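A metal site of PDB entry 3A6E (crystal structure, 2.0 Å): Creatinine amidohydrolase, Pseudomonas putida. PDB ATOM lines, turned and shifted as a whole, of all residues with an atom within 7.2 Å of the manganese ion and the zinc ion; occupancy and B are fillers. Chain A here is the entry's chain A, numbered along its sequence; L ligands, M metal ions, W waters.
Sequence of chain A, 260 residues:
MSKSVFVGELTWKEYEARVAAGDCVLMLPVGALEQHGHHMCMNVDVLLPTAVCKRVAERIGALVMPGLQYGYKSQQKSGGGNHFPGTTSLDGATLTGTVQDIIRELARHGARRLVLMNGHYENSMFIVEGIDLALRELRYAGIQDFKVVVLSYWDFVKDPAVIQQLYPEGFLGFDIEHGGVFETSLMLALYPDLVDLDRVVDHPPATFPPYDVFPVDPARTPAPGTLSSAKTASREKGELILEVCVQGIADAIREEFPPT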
ATOM      1  N   GLY A  31     -22.764  22.037 -10.822  1.00  0.00           N
ATOM      2  CA  GLY A  31     -21.693  22.214 -11.784  1.00  0.00           C
ATOM      3  C   GLY A  31     -20.358  22.671 -11.228  1.00  0.00           C
ATOM      4  O   GLY A  31     -19.876  22.162 -10.221  1.00  0.00           O
ATOM      5  N   ALA A  32     -19.755  23.649 -11.904  1.00  0.00           N
ATOM      6  CA  ALA A  32     -18.457  24.176 -11.485  1.00  0.00           C
ATOM      7  C   ALA A  32     -18.046  25.347 -12.360  1.00  0.00           C
ATOM      8  O   ALA A  32     -18.639  25.580 -13.415  1.00  0.00           O
ATOM      9  CB  ALA A  32     -17.401  23.085 -11.591  1.00  0.00           C
ATOM     10  N   GLU A  34     -14.920  26.221 -14.269  1.00  0.00           N
ATOM     11  CA  GLU A  34     -13.696  25.551 -14.655  1.00  0.00           C
ATOM     12  C   GLU A  34     -13.265  25.833 -16.082  1.00  0.00           C
ATOM     13  O   GLU A  34     -14.106  25.965 -16.985  1.00  0.00           O
ATOM     14  CB  GLU A  34     -13.913  24.043 -14.470  1.00  0.00           C
ATOM     15  CG  GLU A  34     -12.790  23.107 -14.899  1.00  0.00           C
ATOM     16  CD  GLU A  34     -13.236  21.659 -14.841  1.00  0.00           C
ATOM     17  OE1 GLU A  34     -14.312  21.373 -15.381  1.00  0.00           O
ATOM     18  OE2 GLU A  34     -12.524  20.806 -14.262  1.00  0.00           O
ATOM     19  N   GLN A  35     -11.955  25.913 -16.293  1.00  0.00           N
ATOM     20  CA  GLN A  35     -11.417  26.173 -17.614  1.00  0.00           C
ATOM     21  C   GLN A  35     -11.900  25.092 -18.578  1.00  0.00           C
ATOM     22  O   GLN A  35     -11.967  23.909 -18.222  1.00  0.00           O
ATOM     23  CB  GLN A  35      -9.882  26.174 -17.567  1.00  0.00           C
ATOM     24  CG  GLN A  35      -9.225  24.823 -17.241  1.00  0.00           C
ATOM     25  CD  GLN A  35      -9.103  23.908 -18.452  1.00  0.00           C
ATOM     26  OE1 GLN A  35      -9.118  24.356 -19.596  1.00  0.00           O
ATOM     27  NE2 GLN A  35      -8.952  22.605 -18.191  1.00  0.00           N
ATOM     28  N   HIS A  36     -12.273  25.504 -19.785  1.00  0.00           N
ATOM     29  CA  HIS A  36     -12.717  24.579 -20.812  1.00  0.00           C
ATOM     30  C   HIS A  36     -12.028  24.867 -22.131  1.00  0.00           C
ATOM     31  O   HIS A  36     -12.680  25.005 -23.160  1.00  0.00           O
ATOM     32  CB  HIS A  36     -14.238  24.648 -20.986  1.00  0.00           C
ATOM     33  CG  HIS A  36     -14.982  23.763 -20.035  1.00  0.00           C
ATOM     34  ND1 HIS A  36     -15.065  24.036 -18.680  1.00  0.00           N
ATOM     35  CD2 HIS A  36     -15.615  22.586 -20.214  1.00  0.00           C
ATOM     36  CE1 HIS A  36     -15.713  23.053 -18.072  1.00  0.00           C
ATOM     37  NE2 HIS A  36     -16.053  22.159 -18.991  1.00  0.00           N
ATOM     38  N   MET A  40     -14.104  27.557 -25.300  1.00  0.00           N
ATOM     39  CA  MET A  40     -15.370  27.642 -24.580  1.00  0.00           C
ATOM     40  C   MET A  40     -15.237  28.405 -23.267  1.00  0.00           C
ATOM     41  O   MET A  40     -14.145  28.523 -22.728  1.00  0.00           O
ATOM     42  CB  MET A  40     -15.944  26.252 -24.296  1.00  0.00           C
ATOM     43  CG  MET A  40     -16.454  25.512 -25.508  1.00  0.00           C
ATOM     44  SD  MET A  40     -17.505  24.129 -25.028  1.00  0.00           S
ATOM     45  CE  MET A  40     -16.288  22.987 -24.373  1.00  0.00           C
ATOM     46  N   VAL A  44     -19.522  26.142 -18.415  1.00  0.00           N
ATOM     47  CA  VAL A  44     -20.080  25.002 -19.139  1.00  0.00           C
ATOM     48  C   VAL A  44     -20.692  23.923 -18.234  1.00  0.00           C
ATOM     49  O   VAL A  44     -21.785  23.416 -18.505  1.00  0.00           O
ATOM     50  CB  VAL A  44     -18.991  24.327 -20.027  1.00  0.00           C
ATOM     51  CG1 VAL A  44     -19.520  23.019 -20.610  1.00  0.00           C
ATOM     52  CG2 VAL A  44     -18.583  25.284 -21.158  1.00  0.00           C
ATOM     53  N   ASP A  45     -19.991  23.565 -17.150  1.00  0.00           N
ATOM     54  CA  ASP A  45     -20.471  22.535 -16.232  1.00  0.00           C
ATOM     55  C   ASP A  45     -21.742  22.925 -15.480  1.00  0.00           C
ATOM     56  O   ASP A  45     -22.357  22.082 -14.841  1.00  0.00           O
ATOM     57  CB  ASP A  45     -19.382  22.141 -15.241  1.00  0.00           C
ATOM     58  CG  ASP A  45     -18.285  21.318 -15.883  1.00  0.00           C
ATOM     59  OD1 ASP A  45     -18.415  21.008 -17.091  1.00  0.00           O
ATOM     60  OD2 ASP A  45     -17.302  20.983 -15.210  1.00  0.00           O
ATOM     61  N   VAL A  46     -22.103  24.194 -15.548  1.00  0.00           N
ATOM     62  CA  VAL A  46     -23.329  24.666 -14.919  1.00  0.00           C
ATOM     63  C   VAL A  46     -24.382  24.759 -16.017  1.00  0.00           C
ATOM     64  O   VAL A  46     -25.502  24.272 -15.863  1.00  0.00           O
ATOM     65  CB  VAL A  46     -23.182  26.078 -14.298  1.00  0.00           C
ATOM     66  CG1 VAL A  46     -24.569  26.622 -13.924  1.00  0.00           C
ATOM     67  CG2 VAL A  46     -22.303  26.023 -13.067  1.00  0.00           C
ATOM     68  N   LEU A  48     -24.691  23.270 -18.984  1.00  0.00           N
ATOM     69  CA  LEU A  48     -25.173  22.016 -19.556  1.00  0.00           C
ATOM     70  C   LEU A  48     -26.158  21.210 -18.708  1.00  0.00           C
ATOM     71  O   LEU A  48     -27.236  20.874 -19.192  1.00  0.00           O
ATOM     72  CB  LEU A  48     -23.969  21.158 -19.977  1.00  0.00           C
ATOM     73  CG  LEU A  48     -23.169  21.847 -21.090  1.00  0.00           C
ATOM     74  CD1 LEU A  48     -22.079  20.912 -21.614  1.00  0.00           C
ATOM     75  CD2 LEU A  48     -24.111  22.240 -22.237  1.00  0.00           C
ATOM     76  N   TYR A  72     -16.204  20.728  -6.899  1.00  0.00           N
ATOM     77  CA  TYR A  72     -14.937  20.251  -6.367  1.00  0.00           C
ATOM     78  C   TYR A  72     -13.755  20.532  -7.292  1.00  0.00           C
ATOM     79  O   TYR A  72     -13.916  20.741  -8.495  1.00  0.00           O
ATOM     80  CB  TYR A  72     -14.999  18.756  -6.052  1.00  0.00           C
ATOM     81  CG  TYR A  72     -13.775  18.250  -5.313  1.00  0.00           C
ATOM     82  CD1 TYR A  72     -13.479  18.704  -4.022  1.00  0.00           C
ATOM     83  CD2 TYR A  72     -12.868  17.394  -5.942  1.00  0.00           C
ATOM     84  CE1 TYR A  72     -12.309  18.310  -3.376  1.00  0.00           C
ATOM     85  CE2 TYR A  72     -11.690  17.004  -5.298  1.00  0.00           C
ATOM     86  CZ  TYR A  72     -11.418  17.470  -4.026  1.00  0.00           C
ATOM     87  OH  TYR A  72     -10.239  17.105  -3.410  1.00  0.00           O
ATOM     88  N   SER A  74     -10.827  20.620  -9.753  1.00  0.00           N
ATOM     89  CA  SER A  74     -10.614  19.993 -11.053  1.00  0.00           C
ATOM     90  C   SER A  74      -9.423  19.044 -10.932  1.00  0.00           C
ATOM     91  O   SER A  74      -8.391  19.408 -10.370  1.00  0.00           O
ATOM     92  CB  SER A  74     -10.312  21.079 -12.097  1.00  0.00           C
ATOM     93  OG  SER A  74     -10.029  20.519 -13.370  1.00  0.00           O
ATOM     94  N   SER A  78      -9.219  14.367 -15.499  1.00  0.00           N
ATOM     95  CA  SER A  78     -10.634  14.519 -15.822  1.00  0.00           C
ATOM     96  C   SER A  78     -10.997  15.946 -16.239  1.00  0.00           C
ATOM     97  O   SER A  78     -11.802  16.142 -17.147  1.00  0.00           O
ATOM     98  CB  SER A  78     -11.506  14.082 -14.641  1.00  0.00           C
ATOM     99  OG  SER A  78     -11.194  14.799 -13.457  1.00  0.00           O
ATOM    100  N   GLY A  79     -10.389  16.934 -15.597  1.00  0.00           N
ATOM    101  CA  GLY A  79     -10.684  18.317 -15.917  1.00  0.00           C
ATOM    102  C   GLY A  79      -9.475  19.181 -16.239  1.00  0.00           C
ATOM    103  O   GLY A  79      -9.607  20.396 -16.374  1.00  0.00           O
ATOM    104  N   GLY A 119     -22.780  17.836 -13.449  1.00  0.00           N
ATOM    105  CA  GLY A 119     -22.264  18.251 -14.738  1.00  0.00           C
ATOM    106  C   GLY A 119     -20.754  18.400 -14.712  1.00  0.00           C
ATOM    107  O   GLY A 119     -20.142  18.720 -15.731  1.00  0.00           O
ATOM    108  N   HIS A 120     -20.172  18.178 -13.535  1.00  0.00           N
ATOM    109  CA  HIS A 120     -18.730  18.281 -13.301  1.00  0.00           C
ATOM    110  C   HIS A 120     -18.311  16.953 -12.677  1.00  0.00           C
ATOM    111  O   HIS A 120     -18.622  16.688 -11.523  1.00  0.00           O
ATOM    112  CB  HIS A 120     -18.446  19.443 -12.349  1.00  0.00           C
ATOM    113  CG  HIS A 120     -17.006  19.594 -11.945  1.00  0.00           C
ATOM    114  ND1 HIS A 120     -15.986  19.766 -12.856  1.00  0.00           N
ATOM    115  CD2 HIS A 120     -16.434  19.696 -10.723  1.00  0.00           C
ATOM    116  CE1 HIS A 120     -14.852  19.963 -12.214  1.00  0.00           C
ATOM    117  NE2 HIS A 120     -15.093  19.935 -10.915  1.00  0.00           N
ATOM    118  N   TYR A 121     -17.601  16.123 -13.459  1.00  0.00           N
ATOM    119  CA  TYR A 121     -17.168  14.793 -13.034  1.00  0.00           C
ATOM    120  C   TYR A 121     -16.643  14.667 -11.608  1.00  0.00           C
ATOM    121  O   TYR A 121     -17.068  13.779 -10.863  1.00  0.00           O
ATOM    122  CB  TYR A 121     -16.085  14.265 -13.991  1.00  0.00           C
ATOM    123  CG  TYR A 121     -15.714  12.823 -13.742  1.00  0.00           C
ATOM    124  CD1 TYR A 121     -16.613  11.793 -13.996  1.00  0.00           C
ATOM    125  CD2 TYR A 121     -14.450  12.490 -13.243  1.00  0.00           C
ATOM    126  CE1 TYR A 121     -16.274  10.465 -13.771  1.00  0.00           C
ATOM    127  CE2 TYR A 121     -14.106  11.161 -13.005  1.00  0.00           C
ATOM    128  CZ  TYR A 121     -15.020  10.152 -13.272  1.00  0.00           C
ATOM    129  OH  TYR A 121     -14.678   8.836 -13.055  1.00  0.00           O
ATOM    130  N   GLU A 122     -15.731  15.551 -11.228  1.00  0.00           N
ATOM    131  CA  GLU A 122     -15.122  15.533  -9.907  1.00  0.00           C
ATOM    132  C   GLU A 122     -16.074  15.701  -8.703  1.00  0.00           C
ATOM    133  O   GLU A 122     -15.713  15.368  -7.580  1.00  0.00           O
ATOM    134  CB  GLU A 122     -14.008  16.602  -9.825  1.00  0.00           C
ATOM    135  CG  GLU A 122     -12.805  16.319 -10.749  1.00  0.00           C
ATOM    136  CD  GLU A 122     -12.965  16.832 -12.179  1.00  0.00           C
ATOM    137  OE1 GLU A 122     -14.102  16.853 -12.709  1.00  0.00           O
ATOM    138  OE2 GLU A 122     -11.943  17.203 -12.789  1.00  0.00           O
ATOM    139  N   ASN A 123     -17.276  16.224  -8.945  1.00  0.00           N
ATOM    140  CA  ASN A 123     -18.262  16.442  -7.867  1.00  0.00           C
ATOM    141  C   ASN A 123     -18.883  15.189  -7.278  1.00  0.00           C
ATOM    142  O   ASN A 123     -19.276  15.170  -6.099  1.00  0.00           O
ATOM    143  CB  ASN A 123     -19.451  17.278  -8.354  1.00  0.00           C
ATOM    144  CG  ASN A 123     -19.106  18.715  -8.651  1.00  0.00           C
ATOM    145  OD1 ASN A 123     -18.178  19.277  -8.092  1.00  0.00           O
ATOM    146  ND2 ASN A 123     -19.902  19.320  -9.533  1.00  0.00           N
ATOM    147  N   TYR A 153     -25.439  13.527 -16.421  1.00  0.00           N
ATOM    148  CA  TYR A 153     -26.164  13.470 -17.680  1.00  0.00           C
ATOM    149  C   TYR A 153     -25.506  12.720 -18.831  1.00  0.00           C
ATOM    150  O   TYR A 153     -26.197  12.040 -19.593  1.00  0.00           O
ATOM    151  CB  TYR A 153     -26.583  14.892 -18.128  1.00  0.00           C
ATOM    152  CG  TYR A 153     -25.459  15.757 -18.662  1.00  0.00           C
ATOM    153  CD1 TYR A 153     -25.065  15.668 -19.997  1.00  0.00           C
ATOM    154  CD2 TYR A 153     -24.759  16.625 -17.829  1.00  0.00           C
ATOM    155  CE1 TYR A 153     -24.012  16.426 -20.486  1.00  0.00           C
ATOM    156  CE2 TYR A 153     -23.706  17.388 -18.310  1.00  0.00           C
ATOM    157  CZ  TYR A 153     -23.337  17.286 -19.636  1.00  0.00           C
ATOM    158  OH  TYR A 153     -22.261  17.991 -20.104  1.00  0.00           O
ATOM    159  N   TRP A 154     -24.190  12.806 -18.950  1.00  0.00           N
ATOM    160  CA  TRP A 154     -23.496  12.122 -20.036  1.00  0.00           C
ATOM    161  C   TRP A 154     -23.586  10.591 -19.993  1.00  0.00           C
ATOM    162  O   TRP A 154     -23.466   9.931 -21.034  1.00  0.00           O
ATOM    163  CB  TRP A 154     -22.017  12.541 -20.073  1.00  0.00           C
ATOM    164  CG  TRP A 154     -21.265  12.279 -18.804  1.00  0.00           C
ATOM    165  CD1 TRP A 154     -20.760  11.088 -18.373  1.00  0.00           C
ATOM    166  CD2 TRP A 154     -20.949  13.242 -17.786  1.00  0.00           C
ATOM    167  NE1 TRP A 154     -20.147  11.247 -17.152  1.00  0.00           N
ATOM    168  CE2 TRP A 154     -20.251  12.553 -16.766  1.00  0.00           C
ATOM    169  CE3 TRP A 154     -21.190  14.609 -17.635  1.00  0.00           C
ATOM    170  CZ2 TRP A 154     -19.793  13.195 -15.609  1.00  0.00           C
ATOM    171  CZ3 TRP A 154     -20.731  15.251 -16.478  1.00  0.00           C
ATOM    172  CH2 TRP A 154     -20.042  14.536 -15.489  1.00  0.00           C
ATOM    173  N   GLU A 177     -13.041  13.329 -22.320  1.00  0.00           N
ATOM    174  CA  GLU A 177     -14.048  14.309 -22.678  1.00  0.00           C
ATOM    175  C   GLU A 177     -14.194  15.538 -21.781  1.00  0.00           C
ATOM    176  O   GLU A 177     -15.215  15.730 -21.111  1.00  0.00           O
ATOM    177  CB  GLU A 177     -15.422  13.633 -22.824  1.00  0.00           C
ATOM    178  CG  GLU A 177     -15.591  12.786 -24.095  1.00  0.00           C
ATOM    179  CD  GLU A 177     -15.488  13.591 -25.383  1.00  0.00           C
ATOM    180  OE1 GLU A 177     -15.737  14.820 -25.359  1.00  0.00           O
ATOM    181  OE2 GLU A 177     -15.174  12.987 -26.428  1.00  0.00           O
ATOM    182  N   HIS A 178     -13.164  16.380 -21.767  1.00  0.00           N
ATOM    183  CA  HIS A 178     -13.223  17.632 -21.028  1.00  0.00           C
ATOM    184  C   HIS A 178     -12.933  18.685 -22.087  1.00  0.00           C
ATOM    185  O   HIS A 178     -11.799  18.805 -22.543  1.00  0.00           O
ATOM    186  CB  HIS A 178     -12.169  17.721 -19.927  1.00  0.00           C
ATOM    187  CG  HIS A 178     -12.107  19.084 -19.285  1.00  0.00           C
ATOM    188  ND1 HIS A 178     -13.189  19.637 -18.627  1.00  0.00           N
ATOM    189  CD2 HIS A 178     -11.132  20.014 -19.265  1.00  0.00           C
ATOM    190  CE1 HIS A 178     -12.883  20.860 -18.234  1.00  0.00           C
ATOM    191  NE2 HIS A 178     -11.641  21.119 -18.614  1.00  0.00           N
ATOM    192  N   GLY A 179     -13.954  19.430 -22.497  1.00  0.00           N
ATOM    193  CA  GLY A 179     -13.772  20.438 -23.525  1.00  0.00           C
ATOM    194  C   GLY A 179     -13.620  19.793 -24.895  1.00  0.00           C
ATOM    195  O   GLY A 179     -13.174  20.431 -25.850  1.00  0.00           O
ATOM    196  N   GLU A 183     -18.943  17.780 -24.938  1.00  0.00           N
ATOM    197  CA  GLU A 183     -19.422  19.031 -24.355  1.00  0.00           C
ATOM    198  C   GLU A 183     -19.506  20.162 -25.359  1.00  0.00           C
ATOM    199  O   GLU A 183     -20.403  20.987 -25.291  1.00  0.00           O
ATOM    200  CB  GLU A 183     -18.509  19.496 -23.238  1.00  0.00           C
ATOM    201  CG  GLU A 183     -18.418  18.593 -22.047  1.00  0.00           C
ATOM    202  CD  GLU A 183     -17.654  19.248 -20.940  1.00  0.00           C
ATOM    203  OE1 GLU A 183     -18.276  19.609 -19.924  1.00  0.00           O
ATOM    204  OE2 GLU A 183     -16.428  19.431 -21.107  1.00  0.00           O
HETATM  205 AS1  LIG L   1     -16.378  17.441 -17.068  1.00  0.00          AS
HETATM  206  O1  LIG L   1     -16.726  17.662 -15.368  1.00  0.00           O
HETATM  207  O2  LIG L   1     -15.700  18.940 -17.636  1.00  0.00           O
HETATM  208  C1  LIG L   1     -14.999  16.071 -17.337  1.00  0.00           C
HETATM  209  C2  LIG L   1     -18.021  17.116 -18.078  1.00  0.00           C
HETATM  210 MN    MN M   1     -15.665  19.636 -15.074  1.00  0.00          MN
HETATM  211 ZN    ZN M   2     -17.007  20.348 -18.492  1.00  0.00          ZN
HETATM  212  O   HOH W   1     -13.920  18.406 -14.966  1.00  0.00           O
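The zinc ion is bound by OE1 of Glu 183 (2.1 Å), OD1 of Asp 45 (2.1 Å), O2 of the ligand (2.1 Å) and NE2 of His 36 (2.1 Å).
Slightly farther from the zinc ion lies the side-chain carboxylate (OE2) of Glu 183 (2.8 Å).
The manganese ion is bound by the side-chain carboxylate of Asp 45 (2.1 Å), water W1 (2.1 Å), the side-chain carboxylate of Glu 34 (2.2 Å), a ring nitrogen (ND1) of His 120 (2.2 Å), an oxygen (O1) of the ligand (2.3 Å) and an oxygen (O2) of the ligand (2.7 Å).
Residues that only touch the zinc ion: His 178.
The side-chain carboxylate of Glu 122 lies within hydrogen-bond range of the side-chain hydroxyl of Ser 78, 2.6 Å away.
O of Glu 34 sits at hydrogen-bond distance from ND1 of His 36, at 2.7 Å.
A ring nitrogen (ND1) of His 120 lies close to the side-chain carboxylate of Glu 122, 3.5 Å away.
The side-chain carboxylate of Glu 122 sits at hydrogen-bond distance from the backbone NH of Gly 79 (3.2 Å).
NE2 of His 178 lies within hydrogen-bond range of O of Gly 79 (3.1 Å).
OE2 of Glu 34 is in hydrogen-bond range of OG of Ser 74 (2.7 Å).
The backbone carbonyl oxygen of Tyr 72 sits at hydrogen-bond distance from a ring nitrogen (NE2) of His 120 (2.8 Å).
A ring nitrogen (NE2) of His 178 lies within hydrogen-bond range of the backbone carbonyl oxygen of Gln 35 (2.8 Å).
Glu 122 touches the manganese ion.
Of the 25 residues printed, 4 come within 4 Å of the manganese ion.
Water W1 lies within hydrogen-bond range of the side-chain carboxylate of Glu 122 (2.7 Å) and the side-chain carboxylate of Glu 34 (2.9 Å).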
